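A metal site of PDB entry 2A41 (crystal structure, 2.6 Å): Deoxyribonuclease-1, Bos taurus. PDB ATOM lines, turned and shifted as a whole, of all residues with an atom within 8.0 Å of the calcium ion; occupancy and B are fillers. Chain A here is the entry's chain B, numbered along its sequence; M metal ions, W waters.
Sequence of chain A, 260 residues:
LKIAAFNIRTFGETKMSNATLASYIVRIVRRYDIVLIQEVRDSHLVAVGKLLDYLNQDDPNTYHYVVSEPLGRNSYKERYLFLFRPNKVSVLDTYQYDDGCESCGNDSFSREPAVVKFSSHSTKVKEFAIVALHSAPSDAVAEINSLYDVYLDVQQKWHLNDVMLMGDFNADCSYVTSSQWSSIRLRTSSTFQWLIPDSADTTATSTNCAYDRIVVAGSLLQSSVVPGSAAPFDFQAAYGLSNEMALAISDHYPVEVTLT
The side-chain hydroxyl (OG1) of Thr 205 sits at hydrogen-bond distance from the side-chain hydroxyl (OG1) of Thr 207 (3.1 Å). The side-chain hydroxyl (OH) of Tyr 253 sits close to the backbone carbonyl oxygen (O) of Thr 203.
The calcium ion is bound by water W2 (2.4 Å), the backbone carbonyl oxygen (O) of Thr 207 (2.4 Å), the backbone carbonyl oxygen (O) of Thr 203 (2.4 Å), the side-chain carboxylate (OD2) of Asp 201 (2.4 Å), the backbone carbonyl oxygen (O) of Thr 205 (2.5 Å), water W1 (2.5 Å), the side-chain carboxylate (OD1) of Asp 201 (2.5 Å) and the side-chain hydroxyl (OG1) of Thr 203 (2.5 Å). The calcium ion has eight donor atoms within binding distance.
Four residues have an atom within 4 Å of the calcium ion: Asp 201, Thr 203, Thr 205 and Thr 207.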
ATOM      1  N   ALA A 200      17.797 -20.890 -16.350  1.00  0.00           N
ATOM      2  CA  ALA A 200      18.646 -21.826 -17.092  1.00  0.00           C
ATOM      3  C   ALA A 200      19.037 -21.310 -18.488  1.00  0.00           C
ATOM      4  O   ALA A 200      18.198 -20.763 -19.202  1.00  0.00           O
ATOM      5  CB  ALA A 200      17.961 -23.159 -17.202  1.00  0.00           C
ATOM      6  N   ASP A 201      20.310 -21.475 -18.851  1.00  0.00           N
ATOM      7  CA  ASP A 201      20.748 -21.280 -20.235  1.00  0.00           C
ATOM      8  C   ASP A 201      20.693 -22.607 -20.992  1.00  0.00           C
ATOM      9  O   ASP A 201      21.488 -23.504 -20.726  1.00  0.00           O
ATOM     10  CB  ASP A 201      22.154 -20.672 -20.312  1.00  0.00           C
ATOM     11  CG  ASP A 201      22.708 -20.614 -21.759  1.00  0.00           C
ATOM     12  OD1 ASP A 201      21.941 -20.694 -22.759  1.00  0.00           O
ATOM     13  OD2 ASP A 201      23.926 -20.472 -21.898  1.00  0.00           O
ATOM     14  N   THR A 202      19.766 -22.745 -21.928  1.00  0.00           N
ATOM     15  CA  THR A 202      19.720 -23.981 -22.698  1.00  0.00           C
ATOM     16  C   THR A 202      20.187 -23.829 -24.154  1.00  0.00           C
ATOM     17  O   THR A 202      20.002 -24.750 -24.963  1.00  0.00           O
ATOM     18  CB  THR A 202      18.324 -24.617 -22.694  1.00  0.00           C
ATOM     19  OG1 THR A 202      17.526 -24.008 -23.720  1.00  0.00           O
ATOM     20  CG2 THR A 202      17.649 -24.486 -21.336  1.00  0.00           C
ATOM     21  N   THR A 203      20.787 -22.692 -24.490  1.00  0.00           N
ATOM     22  CA  THR A 203      21.321 -22.512 -25.843  1.00  0.00           C
ATOM     23  C   THR A 203      22.829 -22.695 -25.859  1.00  0.00           C
ATOM     24  O   THR A 203      23.537 -22.257 -24.914  1.00  0.00           O
ATOM     25  CB  THR A 203      20.989 -21.137 -26.422  1.00  0.00           C
ATOM     26  OG1 THR A 203      21.769 -20.141 -25.770  1.00  0.00           O
ATOM     27  CG2 THR A 203      19.510 -20.808 -26.239  1.00  0.00           C
ATOM     28  N   ALA A 204      23.331 -23.330 -26.925  1.00  0.00           N
ATOM     29  CA  ALA A 204      24.765 -23.442 -27.112  1.00  0.00           C
ATOM     30  C   ALA A 204      25.351 -22.161 -27.706  1.00  0.00           C
ATOM     31  O   ALA A 204      26.542 -22.068 -27.948  1.00  0.00           O
ATOM     32  CB  ALA A 204      25.096 -24.625 -27.998  1.00  0.00           C
ATOM     33  N   THR A 205      24.500 -21.161 -27.929  1.00  0.00           N
ATOM     34  CA  THR A 205      24.916 -19.920 -28.557  1.00  0.00           C
ATOM     35  C   THR A 205      25.102 -18.840 -27.506  1.00  0.00           C
ATOM     36  O   THR A 205      24.795 -19.041 -26.335  1.00  0.00           O
ATOM     37  CB  THR A 205      23.820 -19.428 -29.534  1.00  0.00           C
ATOM     38  OG1 THR A 205      22.572 -19.313 -28.822  1.00  0.00           O
ATOM     39  CG2 THR A 205      23.625 -20.408 -30.665  1.00  0.00           C
ATOM     40  N   SER A 206      25.596 -17.702 -27.947  1.00  0.00           N
ATOM     41  CA  SER A 206      25.677 -16.475 -27.180  1.00  0.00           C
ATOM     42  C   SER A 206      24.492 -16.054 -26.327  1.00  0.00           C
ATOM     43  O   SER A 206      24.651 -15.214 -25.447  1.00  0.00           O
ATOM     44  CB  SER A 206      25.836 -15.344 -28.159  1.00  0.00           C
ATOM     45  OG  SER A 206      27.177 -15.239 -28.491  1.00  0.00           O
ATOM     46  N   THR A 207      23.288 -16.539 -26.650  1.00  0.00           N
ATOM     47  CA  THR A 207      22.118 -16.082 -25.929  1.00  0.00           C
ATOM     48  C   THR A 207      21.995 -16.772 -24.591  1.00  0.00           C
ATOM     49  O   THR A 207      22.441 -17.918 -24.433  1.00  0.00           O
ATOM     50  CB  THR A 207      20.813 -16.316 -26.723  1.00  0.00           C
ATOM     51  OG1 THR A 207      20.677 -17.715 -27.040  1.00  0.00           O
ATOM     52  CG2 THR A 207      20.825 -15.480 -28.004  1.00  0.00           C
ATOM     53  N   ASN A 208      21.402 -16.077 -23.625  1.00  0.00           N
ATOM     54  CA  ASN A 208      21.062 -16.682 -22.321  1.00  0.00           C
ATOM     55  C   ASN A 208      19.560 -16.979 -22.237  1.00  0.00           C
ATOM     56  O   ASN A 208      18.787 -16.202 -21.706  1.00  0.00           O
ATOM     57  CB  ASN A 208      21.504 -15.783 -21.163  1.00  0.00           C
ATOM     58  CG  ASN A 208      21.086 -16.322 -19.793  1.00  0.00           C
ATOM     59  OD1 ASN A 208      21.083 -17.541 -19.569  1.00  0.00           O
ATOM     60  ND2 ASN A 208      20.726 -15.411 -18.883  1.00  0.00           N
ATOM     61  N   CYS A 209      19.145 -18.121 -22.770  1.00  0.00           N
ATOM     62  CA  CYS A 209      17.723 -18.405 -22.861  1.00  0.00           C
ATOM     63  C   CYS A 209      17.351 -19.784 -22.337  1.00  0.00           C
ATOM     64  O   CYS A 209      17.925 -20.779 -22.747  1.00  0.00           O
ATOM     65  CB  CYS A 209      17.229 -18.283 -24.306  1.00  0.00           C
ATOM     66  SG  CYS A 209      17.560 -16.679 -25.129  1.00  0.00           S
ATOM     67  N   ALA A 210      16.384 -19.831 -21.426  1.00  0.00           N
ATOM     68  CA  ALA A 210      15.710 -21.076 -21.054  1.00  0.00           C
ATOM     69  C   ALA A 210      14.664 -21.487 -22.118  1.00  0.00           C
ATOM     70  O   ALA A 210      13.461 -21.506 -21.864  1.00  0.00           O
ATOM     71  CB  ALA A 210      15.045 -20.938 -19.691  1.00  0.00           C
ATOM     72  N   ASN A 243      33.918 -23.533 -29.214  1.00  0.00           N
ATOM     73  CA  ASN A 243      32.504 -23.171 -29.443  1.00  0.00           C
ATOM     74  C   ASN A 243      32.041 -23.531 -30.864  1.00  0.00           C
ATOM     75  O   ASN A 243      30.928 -23.983 -31.082  1.00  0.00           O
ATOM     76  CB  ASN A 243      32.223 -21.692 -29.144  1.00  0.00           C
ATOM     77  CG  ASN A 243      30.725 -21.427 -29.002  1.00  0.00           C
ATOM     78  OD1 ASN A 243      30.134 -20.639 -29.743  1.00  0.00           O
ATOM     79  ND2 ASN A 243      30.098 -22.135 -28.056  1.00  0.00           N
ATOM     80  N   LEU A 247      28.645 -25.639 -31.616  1.00  0.00           N
ATOM     81  CA  LEU A 247      27.636 -25.141 -32.534  1.00  0.00           C
ATOM     82  C   LEU A 247      27.417 -26.059 -33.740  1.00  0.00           C
ATOM     83  O   LEU A 247      26.290 -26.137 -34.252  1.00  0.00           O
ATOM     84  CB  LEU A 247      28.026 -23.730 -32.993  1.00  0.00           C
ATOM     85  CG  LEU A 247      27.315 -22.472 -32.481  1.00  0.00           C
ATOM     86  CD1 LEU A 247      26.473 -22.686 -31.228  1.00  0.00           C
ATOM     87  CD2 LEU A 247      28.303 -21.340 -32.296  1.00  0.00           C
ATOM     88  N   ASP A 251      22.593 -25.888 -31.764  1.00  0.00           N
ATOM     89  CA  ASP A 251      22.600 -24.650 -31.050  1.00  0.00           C
ATOM     90  C   ASP A 251      21.791 -24.760 -29.762  1.00  0.00           C
ATOM     91  O   ASP A 251      21.592 -23.770 -29.077  1.00  0.00           O
ATOM     92  CB  ASP A 251      22.319 -23.421 -31.935  1.00  0.00           C
ATOM     93  CG  ASP A 251      21.022 -23.523 -32.722  1.00  0.00           C
ATOM     94  OD1 ASP A 251      20.492 -24.656 -32.839  1.00  0.00           O
ATOM     95  OD2 ASP A 251      20.525 -22.476 -33.211  1.00  0.00           O
ATOM     96  N   HIS A 252      21.370 -25.972 -29.402  1.00  0.00           N
ATOM     97  CA  HIS A 252      20.809 -26.228 -28.060  1.00  0.00           C
ATOM     98  C   HIS A 252      21.525 -27.315 -27.288  1.00  0.00           C
ATOM     99  O   HIS A 252      22.048 -28.277 -27.865  1.00  0.00           O
ATOM    100  CB  HIS A 252      19.338 -26.607 -28.091  1.00  0.00           C
ATOM    101  CG  HIS A 252      18.467 -25.620 -28.805  1.00  0.00           C
ATOM    102  ND1 HIS A 252      17.590 -24.796 -28.151  1.00  0.00           N
ATOM    103  CD2 HIS A 252      18.349 -25.328 -30.123  1.00  0.00           C
ATOM    104  CE1 HIS A 252      16.966 -24.032 -29.035  1.00  0.00           C
ATOM    105  NE2 HIS A 252      17.408 -24.344 -30.235  1.00  0.00           N
ATOM    106  N   TYR A 253      21.529 -27.158 -25.970  1.00  0.00           N
ATOM    107  CA  TYR A 253      21.846 -28.240 -25.097  1.00  0.00           C
ATOM    108  C   TYR A 253      20.614 -29.115 -24.874  1.00  0.00           C
ATOM    109  O   TYR A 253      19.476 -28.639 -24.867  1.00  0.00           O
ATOM    110  CB  TYR A 253      22.261 -27.709 -23.737  1.00  0.00           C
ATOM    111  CG  TYR A 253      23.370 -26.683 -23.775  1.00  0.00           C
ATOM    112  CD1 TYR A 253      24.481 -26.850 -24.604  1.00  0.00           C
ATOM    113  CD2 TYR A 253      23.331 -25.565 -22.953  1.00  0.00           C
ATOM    114  CE1 TYR A 253      25.503 -25.918 -24.616  1.00  0.00           C
ATOM    115  CE2 TYR A 253      24.344 -24.650 -22.980  1.00  0.00           C
ATOM    116  CZ  TYR A 253      25.424 -24.831 -23.803  1.00  0.00           C
ATOM    117  OH  TYR A 253      26.421 -23.904 -23.816  1.00  0.00           O
HETATM  118 CA    CA M   1      23.763 -19.913 -24.276  1.00  0.00          CA
HETATM  119  O   HOH W   1      25.282 -18.240 -23.283  1.00  0.00           O
HETATM  120  O   HOH W   2      25.856 -20.984 -23.879  1.00  0.00           O
